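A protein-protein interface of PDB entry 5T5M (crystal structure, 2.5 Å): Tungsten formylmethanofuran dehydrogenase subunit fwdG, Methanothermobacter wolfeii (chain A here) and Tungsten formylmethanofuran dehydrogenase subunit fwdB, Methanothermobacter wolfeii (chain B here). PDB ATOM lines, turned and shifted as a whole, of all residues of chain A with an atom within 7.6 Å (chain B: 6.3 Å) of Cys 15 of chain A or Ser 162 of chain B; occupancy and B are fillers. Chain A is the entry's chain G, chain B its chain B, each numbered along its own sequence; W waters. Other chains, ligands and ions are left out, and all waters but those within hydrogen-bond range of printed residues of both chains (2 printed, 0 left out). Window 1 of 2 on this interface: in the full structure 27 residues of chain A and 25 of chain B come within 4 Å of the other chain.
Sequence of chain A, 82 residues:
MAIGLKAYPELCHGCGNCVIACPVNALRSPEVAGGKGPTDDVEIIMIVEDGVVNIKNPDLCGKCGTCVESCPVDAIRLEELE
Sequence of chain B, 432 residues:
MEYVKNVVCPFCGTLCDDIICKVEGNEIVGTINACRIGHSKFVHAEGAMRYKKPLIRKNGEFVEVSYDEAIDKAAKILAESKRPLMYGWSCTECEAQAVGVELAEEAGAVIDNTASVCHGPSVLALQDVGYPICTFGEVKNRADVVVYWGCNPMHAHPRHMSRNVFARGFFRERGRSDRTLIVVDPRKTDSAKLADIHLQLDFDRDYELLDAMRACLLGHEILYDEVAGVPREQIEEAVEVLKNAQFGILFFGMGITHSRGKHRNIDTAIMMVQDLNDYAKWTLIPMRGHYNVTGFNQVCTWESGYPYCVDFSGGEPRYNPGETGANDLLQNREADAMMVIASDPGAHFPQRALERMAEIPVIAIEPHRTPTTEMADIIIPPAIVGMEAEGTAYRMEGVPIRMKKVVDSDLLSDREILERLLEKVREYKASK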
ATOM      1  N   CYS A  12      34.259 -24.723   6.711  1.00  0.00           N
ATOM      2  CA  CYS A  12      33.221 -24.221   5.826  1.00  0.00           C
ATOM      3  C   CYS A  12      33.097 -25.069   4.567  1.00  0.00           C
ATOM      4  O   CYS A  12      34.096 -25.487   3.976  1.00  0.00           O
ATOM      5  CB  CYS A  12      33.539 -22.763   5.468  1.00  0.00           C
ATOM      6  SG  CYS A  12      32.810 -22.105   3.961  1.00  0.00           S
ATOM      7  N   HIS A  13      31.855 -25.317   4.156  1.00  0.00           N
ATOM      8  CA  HIS A  13      31.586 -26.042   2.923  1.00  0.00           C
ATOM      9  C   HIS A  13      31.467 -25.112   1.728  1.00  0.00           C
ATOM     10  O   HIS A  13      31.418 -25.592   0.591  1.00  0.00           O
ATOM     11  CB  HIS A  13      30.287 -26.854   3.043  1.00  0.00           C
ATOM     12  CG  HIS A  13      30.338 -27.932   4.077  1.00  0.00           C
ATOM     13  ND1 HIS A  13      29.559 -29.066   4.002  1.00  0.00           N
ATOM     14  CD2 HIS A  13      31.072 -28.053   5.208  1.00  0.00           C
ATOM     15  CE1 HIS A  13      29.815 -29.840   5.041  1.00  0.00           C
ATOM     16  NE2 HIS A  13      30.728 -29.247   5.791  1.00  0.00           N
ATOM     17  N   GLY A  14      31.427 -23.803   1.961  1.00  0.00           N
ATOM     18  CA  GLY A  14      31.168 -22.871   0.885  1.00  0.00           C
ATOM     19  C   GLY A  14      29.770 -23.018   0.342  1.00  0.00           C
ATOM     20  O   GLY A  14      29.532 -22.728  -0.834  1.00  0.00           O
ATOM     21  N   CYS A  15      28.837 -23.463   1.184  1.00  0.00           N
ATOM     22  CA  CYS A  15      27.502 -23.799   0.719  1.00  0.00           C
ATOM     23  C   CYS A  15      26.662 -22.563   0.411  1.00  0.00           C
ATOM     24  O   CYS A  15      25.702 -22.657  -0.358  1.00  0.00           O
ATOM     25  CB  CYS A  15      26.817 -24.667   1.778  1.00  0.00           C
ATOM     26  SG  CYS A  15      25.980 -23.737   3.090  1.00  0.00           S
ATOM     27  N   GLY A  16      26.986 -21.418   1.007  1.00  0.00           N
ATOM     28  CA  GLY A  16      26.325 -20.181   0.676  1.00  0.00           C
ATOM     29  C   GLY A  16      25.103 -19.854   1.503  1.00  0.00           C
ATOM     30  O   GLY A  16      24.539 -18.767   1.326  1.00  0.00           O
ATOM     31  N   ASN A  17      24.665 -20.755   2.392  1.00  0.00           N
ATOM     32  CA  ASN A  17      23.491 -20.463   3.212  1.00  0.00           C
ATOM     33  C   ASN A  17      23.610 -19.082   3.842  1.00  0.00           C
ATOM     34  O   ASN A  17      22.700 -18.252   3.740  1.00  0.00           O
ATOM     35  CB  ASN A  17      23.317 -21.526   4.300  1.00  0.00           C
ATOM     36  CG  ASN A  17      22.892 -22.869   3.745  1.00  0.00           C
ATOM     37  OD1 ASN A  17      22.805 -23.048   2.534  1.00  0.00           O
ATOM     38  ND2 ASN A  17      22.632 -23.826   4.634  1.00  0.00           N
ATOM     39  N   CYS A  18      24.746 -18.821   4.487  1.00  0.00           N
ATOM     40  CA  CYS A  18      24.923 -17.583   5.237  1.00  0.00           C
ATOM     41  C   CYS A  18      24.808 -16.367   4.325  1.00  0.00           C
ATOM     42  O   CYS A  18      24.122 -15.394   4.655  1.00  0.00           O
ATOM     43  CB  CYS A  18      26.278 -17.611   5.942  1.00  0.00           C
ATOM     44  SG  CYS A  18      27.680 -17.458   4.839  1.00  0.00           S
ATOM     45  N   VAL A  19      25.460 -16.411   3.163  1.00  0.00           N
ATOM     46  CA  VAL A  19      25.429 -15.275   2.251  1.00  0.00           C
ATOM     47  C   VAL A  19      23.994 -14.940   1.865  1.00  0.00           C
ATOM     48  O   VAL A  19      23.616 -13.762   1.788  1.00  0.00           O
ATOM     49  CB  VAL A  19      26.291 -15.560   1.009  1.00  0.00           C
ATOM     50  CG1 VAL A  19      26.177 -14.412   0.021  1.00  0.00           C
ATOM     51  CG2 VAL A  19      27.747 -15.785   1.403  1.00  0.00           C
ATOM     52  N   ILE A  20      23.179 -15.965   1.599  1.00  0.00           N
ATOM     53  CA  ILE A  20      21.812 -15.737   1.144  1.00  0.00           C
ATOM     54  C   ILE A  20      20.932 -15.270   2.295  1.00  0.00           C
ATOM     55  O   ILE A  20      20.105 -14.360   2.136  1.00  0.00           O
ATOM     56  CB  ILE A  20      21.255 -17.019   0.498  1.00  0.00           C
ATOM     57  CG1 ILE A  20      22.172 -17.509  -0.633  1.00  0.00           C
ATOM     58  CG2 ILE A  20      19.843 -16.789   0.005  1.00  0.00           C
ATOM     59  CD1 ILE A  20      22.628 -16.420  -1.599  1.00  0.00           C
ATOM     60  N   ALA A  21      21.078 -15.896   3.466  1.00  0.00           N
ATOM     61  CA  ALA A  21      20.216 -15.578   4.600  1.00  0.00           C
ATOM     62  C   ALA A  21      20.436 -14.156   5.102  1.00  0.00           C
ATOM     63  O   ALA A  21      19.522 -13.544   5.667  1.00  0.00           O
ATOM     64  CB  ALA A  21      20.459 -16.582   5.732  1.00  0.00           C
ATOM     65  N   VAL A  32      21.739 -12.103  -4.617  1.00  0.00           N
ATOM     66  CA  VAL A  32      21.859 -12.772  -3.322  1.00  0.00           C
ATOM     67  C   VAL A  32      20.486 -13.018  -2.726  1.00  0.00           C
ATOM     68  O   VAL A  32      20.184 -14.114  -2.240  1.00  0.00           O
ATOM     69  CB  VAL A  32      22.727 -11.936  -2.368  1.00  0.00           C
ATOM     70  CG1 VAL A  32      22.654 -12.492  -0.957  1.00  0.00           C
ATOM     71  CG2 VAL A  32      24.167 -11.878  -2.863  1.00  0.00           C
ATOM     72  N   ALA A  33      19.645 -11.983  -2.713  1.00  0.00           N
ATOM     73  CA  ALA A  33      18.300 -12.130  -2.178  1.00  0.00           C
ATOM     74  C   ALA A  33      17.619 -13.367  -2.745  1.00  0.00           C
ATOM     75  O   ALA A  33      16.857 -14.045  -2.043  1.00  0.00           O
ATOM     76  CB  ALA A  33      17.490 -10.870  -2.485  1.00  0.00           C
ATOM     77  N   GLY A  34      17.904 -13.691  -4.003  1.00  0.00           N
ATOM     78  CA  GLY A  34      17.284 -14.822  -4.675  1.00  0.00           C
ATOM     79  C   GLY A  34      18.086 -16.104  -4.655  1.00  0.00           C
ATOM     80  O   GLY A  34      17.834 -17.016  -5.451  1.00  0.00           O
ATOM     81  N   GLY A  35      19.058 -16.196  -3.757  1.00  0.00           N
ATOM     82  CA  GLY A  35      19.819 -17.414  -3.584  1.00  0.00           C
ATOM     83  C   GLY A  35      21.018 -17.561  -4.489  1.00  0.00           C
ATOM     84  O   GLY A  35      21.669 -18.613  -4.457  1.00  0.00           O
ATOM     85  N   LYS A  36      21.322 -16.556  -5.300  1.00  0.00           N
ATOM     86  CA  LYS A  36      22.454 -16.595  -6.209  1.00  0.00           C
ATOM     87  C   LYS A  36      23.647 -15.883  -5.593  1.00  0.00           C
ATOM     88  O   LYS A  36      23.499 -14.950  -4.802  1.00  0.00           O
ATOM     89  CB  LYS A  36      22.106 -15.932  -7.538  1.00  0.00           C
ATOM     90  CG  LYS A  36      21.064 -16.655  -8.351  1.00  0.00           C
ATOM     91  CD  LYS A  36      20.607 -15.772  -9.471  1.00  0.00           C
ATOM     92  CE  LYS A  36      19.734 -16.511 -10.454  1.00  0.00           C
ATOM     93  NZ  LYS A  36      19.416 -15.609 -11.609  1.00  0.00           N
ATOM     94  N   GLY A  37      24.839 -16.330  -5.963  1.00  0.00           N
ATOM     95  CA  GLY A  37      26.025 -15.567  -5.680  1.00  0.00           C
ATOM     96  C   GLY A  37      25.994 -14.305  -6.514  1.00  0.00           C
ATOM     97  O   GLY A  37      25.497 -14.309  -7.648  1.00  0.00           O
ATOM     98  N   VAL A  48      31.334 -16.323  -0.603  1.00  0.00           N
ATOM     99  CA  VAL A  48      32.157 -17.517  -0.725  1.00  0.00           C
ATOM    100  C   VAL A  48      33.220 -17.214  -1.770  1.00  0.00           C
ATOM    101  O   VAL A  48      32.901 -16.927  -2.929  1.00  0.00           O
ATOM    102  CB  VAL A  48      31.313 -18.740  -1.115  1.00  0.00           C
ATOM    103  CG1 VAL A  48      32.195 -19.955  -1.318  1.00  0.00           C
ATOM    104  CG2 VAL A  48      30.251 -19.018  -0.049  1.00  0.00           C
ATOM    105  N   GLY A  51      36.102 -21.086  -2.497  1.00  0.00           N
ATOM    106  CA  GLY A  51      35.424 -22.216  -1.906  1.00  0.00           C
ATOM    107  C   GLY A  51      35.053 -22.078  -0.444  1.00  0.00           C
ATOM    108  O   GLY A  51      34.510 -23.028   0.129  1.00  0.00           O
ATOM    109  N   VAL A  52      35.312 -20.935   0.184  1.00  0.00           N
ATOM    110  CA  VAL A  52      35.012 -20.765   1.599  1.00  0.00           C
ATOM    111  C   VAL A  52      34.479 -19.363   1.852  1.00  0.00           C
ATOM    112  O   VAL A  52      34.766 -18.417   1.112  1.00  0.00           O
ATOM    113  CB  VAL A  52      36.248 -21.017   2.482  1.00  0.00           C
ATOM    114  CG1 VAL A  52      36.591 -22.485   2.504  1.00  0.00           C
ATOM    115  CG2 VAL A  52      37.421 -20.192   1.980  1.00  0.00           C
ATOM    116  N   VAL A  53      33.699 -19.240   2.928  1.00  0.00           N
ATOM    117  CA  VAL A  53      33.158 -17.947   3.320  1.00  0.00           C
ATOM    118  C   VAL A  53      34.298 -16.994   3.638  1.00  0.00           C
ATOM    119  O   VAL A  53      35.283 -17.371   4.285  1.00  0.00           O
ATOM    120  CB  VAL A  53      32.221 -18.118   4.525  1.00  0.00           C
ATOM    121  CG1 VAL A  53      32.989 -18.663   5.727  1.00  0.00           C
ATOM    122  CG2 VAL A  53      31.532 -16.808   4.867  1.00  0.00           C
ATOM    123  N   SER A  70      21.961 -20.381  10.284  1.00  0.00           N
ATOM    124  CA  SER A  70      21.780 -21.051   9.009  1.00  0.00           C
ATOM    125  C   SER A  70      22.962 -21.930   8.641  1.00  0.00           C
ATOM    126  O   SER A  70      22.922 -22.596   7.601  1.00  0.00           O
ATOM    127  CB  SER A  70      21.547 -20.012   7.906  1.00  0.00           C
ATOM    128  OG  SER A  70      22.758 -19.349   7.604  1.00  0.00           O
ATOM    129  N   CYS A  71      24.014 -21.941   9.460  1.00  0.00           N
ATOM    130  CA  CYS A  71      25.166 -22.794   9.226  1.00  0.00           C
ATOM    131  C   CYS A  71      25.136 -23.981  10.176  1.00  0.00           C
ATOM    132  O   CYS A  71      25.099 -23.784  11.403  1.00  0.00           O
ATOM    133  CB  CYS A  71      26.454 -22.022   9.411  1.00  0.00           C
ATOM    134  SG  CYS A  71      27.867 -23.110   9.551  1.00  0.00           S
ATOM    135  N   PRO A  72      25.187 -25.216   9.668  1.00  0.00           N
ATOM    136  CA  PRO A  72      25.154 -26.388  10.542  1.00  0.00           C
ATOM    137  C   PRO A  72      26.512 -26.846  11.047  1.00  0.00           C
ATOM    138  O   PRO A  72      26.552 -27.746  11.902  1.00  0.00           O
ATOM    139  CB  PRO A  72      24.533 -27.455   9.631  1.00  0.00           C
ATOM    140  CG  PRO A  72      25.023 -27.106   8.278  1.00  0.00           C
ATOM    141  CD  PRO A  72      25.156 -25.596   8.248  1.00  0.00           C
ATOM    142  N   VAL A  73      27.612 -26.268  10.560  1.00  0.00           N
ATOM    143  CA  VAL A  73      28.946 -26.770  10.870  1.00  0.00           C
ATOM    144  C   VAL A  73      29.785 -25.735  11.617  1.00  0.00           C
ATOM    145  O   VAL A  73      31.006 -25.853  11.677  1.00  0.00           O
ATOM    146  CB  VAL A  73      29.670 -27.247   9.598  1.00  0.00           C
ATOM    147  CG1 VAL A  73      28.935 -28.458   8.999  1.00  0.00           C
ATOM    148  CG2 VAL A  73      29.797 -26.105   8.590  1.00  0.00           C
ATOM    149  N   CYS B  35      31.276 -23.599  -4.460  1.00  0.00           N
ATOM    150  CA  CYS B  35      31.423 -24.261  -3.171  1.00  0.00           C
ATOM    151  C   CYS B  35      32.785 -24.952  -3.085  1.00  0.00           C
ATOM    152  O   CYS B  35      33.540 -25.018  -4.057  1.00  0.00           O
ATOM    153  CB  CYS B  35      30.283 -25.258  -2.945  1.00  0.00           C
ATOM    154  SG  CYS B  35      30.416 -26.795  -3.828  1.00  0.00           S
ATOM    155  N   ARG B  36      33.105 -25.460  -1.892  1.00  0.00           N
ATOM    156  CA  ARG B  36      34.425 -26.046  -1.666  1.00  0.00           C
ATOM    157  C   ARG B  36      34.743 -27.143  -2.679  1.00  0.00           C
ATOM    158  O   ARG B  36      35.906 -27.301  -3.067  1.00  0.00           O
ATOM    159  CB  ARG B  36      34.519 -26.596  -0.244  1.00  0.00           C
ATOM    160  CG  ARG B  36      35.816 -27.349   0.053  1.00  0.00           C
ATOM    161  CD  ARG B  36      35.759 -28.038   1.390  1.00  0.00           C
ATOM    162  NE  ARG B  36      35.859 -27.112   2.512  1.00  0.00           N
ATOM    163  CZ  ARG B  36      37.007 -26.637   2.984  1.00  0.00           C
ATOM    164  NH1 ARG B  36      38.156 -26.981   2.425  1.00  0.00           N
ATOM    165  NH2 ARG B  36      37.012 -25.810   4.015  1.00  0.00           N
ATOM    166  N   TYR B 148      14.009 -33.312   1.533  1.00  0.00           N
ATOM    167  CA  TYR B 148      15.219 -33.992   1.095  1.00  0.00           C
ATOM    168  C   TYR B 148      15.139 -35.411   1.642  1.00  0.00           C
ATOM    169  O   TYR B 148      15.365 -35.642   2.835  1.00  0.00           O
ATOM    170  CB  TYR B 148      16.457 -33.271   1.592  1.00  0.00           C
ATOM    171  CG  TYR B 148      16.728 -31.953   0.914  1.00  0.00           C
ATOM    172  CD1 TYR B 148      17.247 -31.910  -0.361  1.00  0.00           C
ATOM    173  CD2 TYR B 148      16.497 -30.758   1.566  1.00  0.00           C
ATOM    174  CE1 TYR B 148      17.507 -30.721  -0.969  1.00  0.00           C
ATOM    175  CE2 TYR B 148      16.758 -29.558   0.960  1.00  0.00           C
ATOM    176  CZ  TYR B 148      17.264 -29.543  -0.302  1.00  0.00           C
ATOM    177  OH  TYR B 148      17.541 -28.336  -0.898  1.00  0.00           O
ATOM    178  N   MET B 154      24.078 -30.755   1.919  1.00  0.00           N
ATOM    179  CA  MET B 154      25.187 -29.998   2.496  1.00  0.00           C
ATOM    180  C   MET B 154      26.540 -30.586   2.104  1.00  0.00           C
ATOM    181  O   MET B 154      27.534 -29.854   2.025  1.00  0.00           O
ATOM    182  CB  MET B 154      25.065 -29.949   4.020  1.00  0.00           C
ATOM    183  CG  MET B 154      24.041 -28.949   4.535  1.00  0.00           C
ATOM    184  SD  MET B 154      24.415 -27.234   4.094  1.00  0.00           S
ATOM    185  CE  MET B 154      26.071 -27.064   4.743  1.00  0.00           C
ATOM    186  N   PRO B 158      26.309 -28.802  -2.376  1.00  0.00           N
ATOM    187  CA  PRO B 158      26.432 -27.859  -1.253  1.00  0.00           C
ATOM    188  C   PRO B 158      25.616 -26.579  -1.399  1.00  0.00           C
ATOM    189  O   PRO B 158      25.080 -26.095  -0.396  1.00  0.00           O
ATOM    190  CB  PRO B 158      27.943 -27.592  -1.198  1.00  0.00           C
ATOM    191  CG  PRO B 158      28.550 -28.894  -1.734  1.00  0.00           C
ATOM    192  CD  PRO B 158      27.626 -29.261  -2.859  1.00  0.00           C
ATOM    193  N   ARG B 159      25.470 -26.027  -2.605  1.00  0.00           N
ATOM    194  CA  ARG B 159      24.725 -24.784  -2.767  1.00  0.00           C
ATOM    195  C   ARG B 159      23.257 -25.015  -3.086  1.00  0.00           C
ATOM    196  O   ARG B 159      22.531 -24.051  -3.350  1.00  0.00           O
ATOM    197  CB  ARG B 159      25.363 -23.923  -3.858  1.00  0.00           C
ATOM    198  CG  ARG B 159      26.815 -23.564  -3.578  1.00  0.00           C
ATOM    199  CD  ARG B 159      27.405 -22.776  -4.725  1.00  0.00           C
ATOM    200  NE  ARG B 159      26.947 -21.389  -4.731  1.00  0.00           N
ATOM    201  CZ  ARG B 159      26.763 -20.661  -5.828  1.00  0.00           C
ATOM    202  NH1 ARG B 159      26.971 -21.178  -7.030  1.00  0.00           N
ATOM    203  NH2 ARG B 159      26.354 -19.407  -5.726  1.00  0.00           N
ATOM    204  N   HIS B 160      22.798 -26.267  -3.037  1.00  0.00           N
ATOM    205  CA  HIS B 160      21.427 -26.581  -3.415  1.00  0.00           C
ATOM    206  C   HIS B 160      20.417 -25.938  -2.463  1.00  0.00           C
ATOM    207  O   HIS B 160      19.418 -25.360  -2.906  1.00  0.00           O
ATOM    208  CB  HIS B 160      21.261 -28.092  -3.456  1.00  0.00           C
ATOM    209  CG  HIS B 160      20.053 -28.550  -4.206  1.00  0.00           C
ATOM    210  ND1 HIS B 160      18.805 -28.628  -3.625  1.00  0.00           N
ATOM    211  CD2 HIS B 160      19.900 -28.965  -5.484  1.00  0.00           C
ATOM    212  CE1 HIS B 160      17.934 -29.073  -4.513  1.00  0.00           C
ATOM    213  NE2 HIS B 160      18.573 -29.289  -5.648  1.00  0.00           N
ATOM    214  N   MET B 161      20.649 -26.031  -1.150  1.00  0.00           N
ATOM    215  CA  MET B 161      19.708 -25.430  -0.202  1.00  0.00           C
ATOM    216  C   MET B 161      19.720 -23.905  -0.291  1.00  0.00           C
ATOM    217  O   MET B 161      18.661 -23.266  -0.266  1.00  0.00           O
ATOM    218  CB  MET B 161      20.018 -25.881   1.229  1.00  0.00           C
ATOM    219  CG  MET B 161      20.101 -27.396   1.399  1.00  0.00           C
ATOM    220  SD  MET B 161      20.382 -27.934   3.097  1.00  0.00           S
ATOM    221  CE  MET B 161      18.805 -27.542   3.827  1.00  0.00           C
ATOM    222  N   SER B 162      20.903 -23.295  -0.387  1.00  0.00           N
ATOM    223  CA  SER B 162      20.942 -21.842  -0.464  1.00  0.00           C
ATOM    224  C   SER B 162      20.232 -21.364  -1.724  1.00  0.00           C
ATOM    225  O   SER B 162      19.525 -20.349  -1.700  1.00  0.00           O
ATOM    226  CB  SER B 162      22.387 -21.339  -0.420  1.00  0.00           C
ATOM    227  OG  SER B 162      23.103 -21.727  -1.568  1.00  0.00           O
ATOM    228  N   ARG B 163      20.362 -22.120  -2.815  1.00  0.00           N
ATOM    229  CA  ARG B 163      19.746 -21.709  -4.064  1.00  0.00           C
ATOM    230  C   ARG B 163      18.242 -21.984  -4.091  1.00  0.00           C
ATOM    231  O   ARG B 163      17.504 -21.255  -4.767  1.00  0.00           O
ATOM    232  CB  ARG B 163      20.445 -22.393  -5.243  1.00  0.00           C
ATOM    233  CG  ARG B 163      21.836 -21.820  -5.573  1.00  0.00           C
ATOM    234  CD  ARG B 163      22.406 -22.428  -6.856  1.00  0.00           C
ATOM    235  NE  ARG B 163      21.477 -22.297  -7.979  1.00  0.00           N
ATOM    236  CZ  ARG B 163      21.550 -22.989  -9.112  1.00  0.00           C
ATOM    237  NH1 ARG B 163      22.510 -23.876  -9.300  1.00  0.00           N
ATOM    238  NH2 ARG B 163      20.651 -22.794 -10.065  1.00  0.00           N
ATOM    239  N   ASN B 164      17.756 -22.992  -3.348  1.00  0.00           N
ATOM    240  CA  ASN B 164      16.346 -23.375  -3.415  1.00  0.00           C
ATOM    241  C   ASN B 164      15.531 -23.136  -2.146  1.00  0.00           C
ATOM    242  O   ASN B 164      14.302 -23.057  -2.239  1.00  0.00           O
ATOM    243  CB  ASN B 164      16.214 -24.864  -3.764  1.00  0.00           C
ATOM    244  CG  ASN B 164      16.552 -25.157  -5.188  1.00  0.00           C
ATOM    245  OD1 ASN B 164      15.831 -24.756  -6.096  1.00  0.00           O
ATOM    246  ND2 ASN B 164      17.647 -25.875  -5.401  1.00  0.00           N
ATOM    247  N   VAL B 165      16.158 -23.063  -0.972  1.00  0.00           N
ATOM    248  CA  VAL B 165      15.443 -22.964   0.301  1.00  0.00           C
ATOM    249  C   VAL B 165      15.645 -21.595   0.952  1.00  0.00           C
ATOM    250  O   VAL B 165      14.677 -20.906   1.279  1.00  0.00           O
ATOM    251  CB  VAL B 165      15.862 -24.098   1.259  1.00  0.00           C
ATOM    252  CG1 VAL B 165      15.068 -24.012   2.553  1.00  0.00           C
ATOM    253  CG2 VAL B 165      15.673 -25.443   0.585  1.00  0.00           C
ATOM    254  N   PHE B 166      16.899 -21.201   1.184  1.00  0.00           N
ATOM    255  CA  PHE B 166      17.146 -19.896   1.781  1.00  0.00           C
ATOM    256  C   PHE B 166      16.835 -18.778   0.804  1.00  0.00           C
ATOM    257  O   PHE B 166      16.484 -17.671   1.224  1.00  0.00           O
ATOM    258  CB  PHE B 166      18.590 -19.809   2.263  1.00  0.00           C
ATOM    259  CG  PHE B 166      18.883 -20.704   3.432  1.00  0.00           C
ATOM    260  CD1 PHE B 166      18.681 -20.255   4.729  1.00  0.00           C
ATOM    261  CD2 PHE B 166      19.338 -22.000   3.237  1.00  0.00           C
ATOM    262  CE1 PHE B 166      18.935 -21.077   5.807  1.00  0.00           C
ATOM    263  CE2 PHE B 166      19.598 -22.822   4.308  1.00  0.00           C
ATOM    264  CZ  PHE B 166      19.397 -22.362   5.596  1.00  0.00           C
ATOM    265  N   ALA B 167      16.931 -19.066  -0.491  1.00  0.00           N
ATOM    266  CA  ALA B 167      16.569 -18.112  -1.530  1.00  0.00           C
ATOM    267  C   ALA B 167      15.164 -17.567  -1.320  1.00  0.00           C
ATOM    268  O   ALA B 167      14.243 -18.296  -0.938  1.00  0.00           O
ATOM    269  CB  ALA B 167      16.649 -18.787  -2.899  1.00  0.00           C
ATOM    270  N   ARG B 168      15.000 -16.277  -1.598  1.00  0.00           N
ATOM    271  CA  ARG B 168      13.690 -15.646  -1.565  1.00  0.00           C
ATOM    272  C   ARG B 168      13.120 -15.651  -2.974  1.00  0.00           C
ATOM    273  O   ARG B 168      13.836 -15.378  -3.940  1.00  0.00           O
ATOM    274  CB  ARG B 168      13.780 -14.225  -1.021  1.00  0.00           C
ATOM    275  CG  ARG B 168      14.454 -14.133   0.336  1.00  0.00           C
ATOM    276  CD  ARG B 168      14.979 -12.733   0.572  1.00  0.00           C
ATOM    277  NE  ARG B 168      15.709 -12.629   1.832  1.00  0.00           N
ATOM    278  CZ  ARG B 168      16.945 -13.075   2.006  1.00  0.00           C
ATOM    279  NH1 ARG B 168      17.590 -13.665   1.010  1.00  0.00           N
ATOM    280  NH2 ARG B 168      17.526 -12.947   3.183  1.00  0.00           N
HETATM  281  O   HOH W   1      23.238 -24.903   0.715  1.00  0.00           O
HETATM  282  O   HOH W   2      28.433 -20.777  -2.320  1.00  0.00           O
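O of Gly 51 of chain A is in hydrogen-bond range of N of Arg 36 of chain B (3.5 Å).
ND1 of His 13 of chain A lies within hydrogen-bond range of O of Met 154 of chain B (2.9 Å).
The backbone carbonyl oxygen (O) of Cys 12 of chain A sits at hydrogen-bond distance from the guanidinium group (NE) of Arg 36 of chain B (2.8 Å).
The backbone carbonyl oxygen (O) of Cys 15 of chain A sits close to the backbone carbonyl oxygen (O) of Pro 158 of chain B, at 3.5 Å.
N of Ser 162 of chain B sits close to OD1 of Asn 17 of chain A, 3.5 Å away.
The backbone carbonyl oxygen of Ala 33 of chain A lies within hydrogen-bond range of the backbone NH of Arg 168 of chain B (2.9 Å).
O of His 13 of chain A lies within hydrogen-bond range of N of Arg 36 of chain B, at 3.0 Å.
NH1 of Arg 168 of chain B lies within hydrogen-bond range of O of Ile 20 of chain A (2.8 Å).
The guanidinium group (NH2) of Arg 168 of chain B is in hydrogen-bond range of the backbone carbonyl oxygen (O) of Ala 21 of chain A (3.2 Å).
OG of Ser 162 of chain B is in hydrogen-bond range of O of Cys 15 of chain A.
The guanidinium group (NH2) of Arg 159 of chain B lies close to the backbone NH (N) of Gly 37 of chain A.
The backbone carbonyl oxygen of Met 161 of chain B sits at hydrogen-bond distance from the backbone NH of Phe 166 of chain B (3.1 Å).
The side-chain amide nitrogen (ND2) of Asn 17 of chain A is in hydrogen-bond range of the backbone carbonyl oxygen (O) of Ser 70 of chain A (3.2 Å).
The side-chain sulfur (SG) of Cys 12 of chain A sits close to the backbone NH (N) of Gly 14 of chain A (3.0 Å).
OD1 of Asn 17 of chain A sits close to SG of Cys 15 of chain A, 3.3 Å away.
SG of Cys 12 of chain A lies close to N of Val 53 of chain A (3.2 Å).
The side-chain hydroxyl (OG) of Ser 162 of chain B is in hydrogen-bond range of the backbone carbonyl oxygen (O) of Arg 159 of chain B.
His 13 of chain A touches Cys 35 of chain B.
O of Cys 15 of chain A touches CA of Arg 159 of chain B (3.4 Å).
ND2 of Asn 17 of chain A touches SD of Met 154 of chain B, 3.9 Å away.
CG1 of Ile 20 of chain A touches CB of Ser 162 of chain B, at 3.8 Å.
Ile 20 of chain A touches Ala 167 of chain B.
Ala 167 of chain B touches Ala 33 of chain A.
Gly 34 of chain A touches Ala 167 of chain B (O to CB, 3.3 Å).
Gly 34 of chain A touches Arg 168 of chain B.
CB of Ala 167 of chain B touches CA of Gly 35 of chain A, at 3.5 Å.
Arg 36 of chain B touches Val 52 of chain A.
Cys 15 of chain A touches just these residues of chain B: Met 154 (3.7 Å), Pro 158 (3.1 Å), Arg 159 (3.4 Å) and Ser 162 (3.0 Å).
Printed residues of chain B within 4 Å of His 13 of chain A: Cys 35, Arg 36 and Met 154.
Of the printed residues of chain B, Gly 14 of chain A touches Cys 35 (3.4 Å) and Arg 159 (3.95 Å).
Val 165 of chain B touches none of the printed residues of chain A.
The nearest printed residue of chain B that does not touch His 13 of chain A is Pro 158 of chain B (4.4 Å).
Hydrophobic or aromatic side chains of chain B within 4 Å of the printed part of chain A: Met 154, Phe 166 and Ala 167.
Of the 24 printed residues of chain A, 16 touch a printed residue of chain B.
Hydrophobic or aromatic side chains of chain A within 4 Å of the printed part of chain B: His 13, Ile 20, Val 52 and Pro 72.
Among the printed residues, no Asp or Glu carboxylate lies within 4 Å of a Lys or Arg side-chain nitrogen of the other chain.
Water W1 lies within hydrogen-bond range of the backbone carbonyl oxygen of Pro 158 of chain B (2.5 Å), the side-chain amide oxygen of Asn 17 of chain A (2.6 Å), the backbone NH of Ser 162 of chain B (3.0 Å) and the backbone NH of Met 161 of chain B (3.4 Å).
Water W2 bridges the backbone carbonyl oxygen (O) of Gly 14 of chain A (2.7 Å) and the guanidinium group (NE) of Arg 159 of chain B (2.9 Å).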
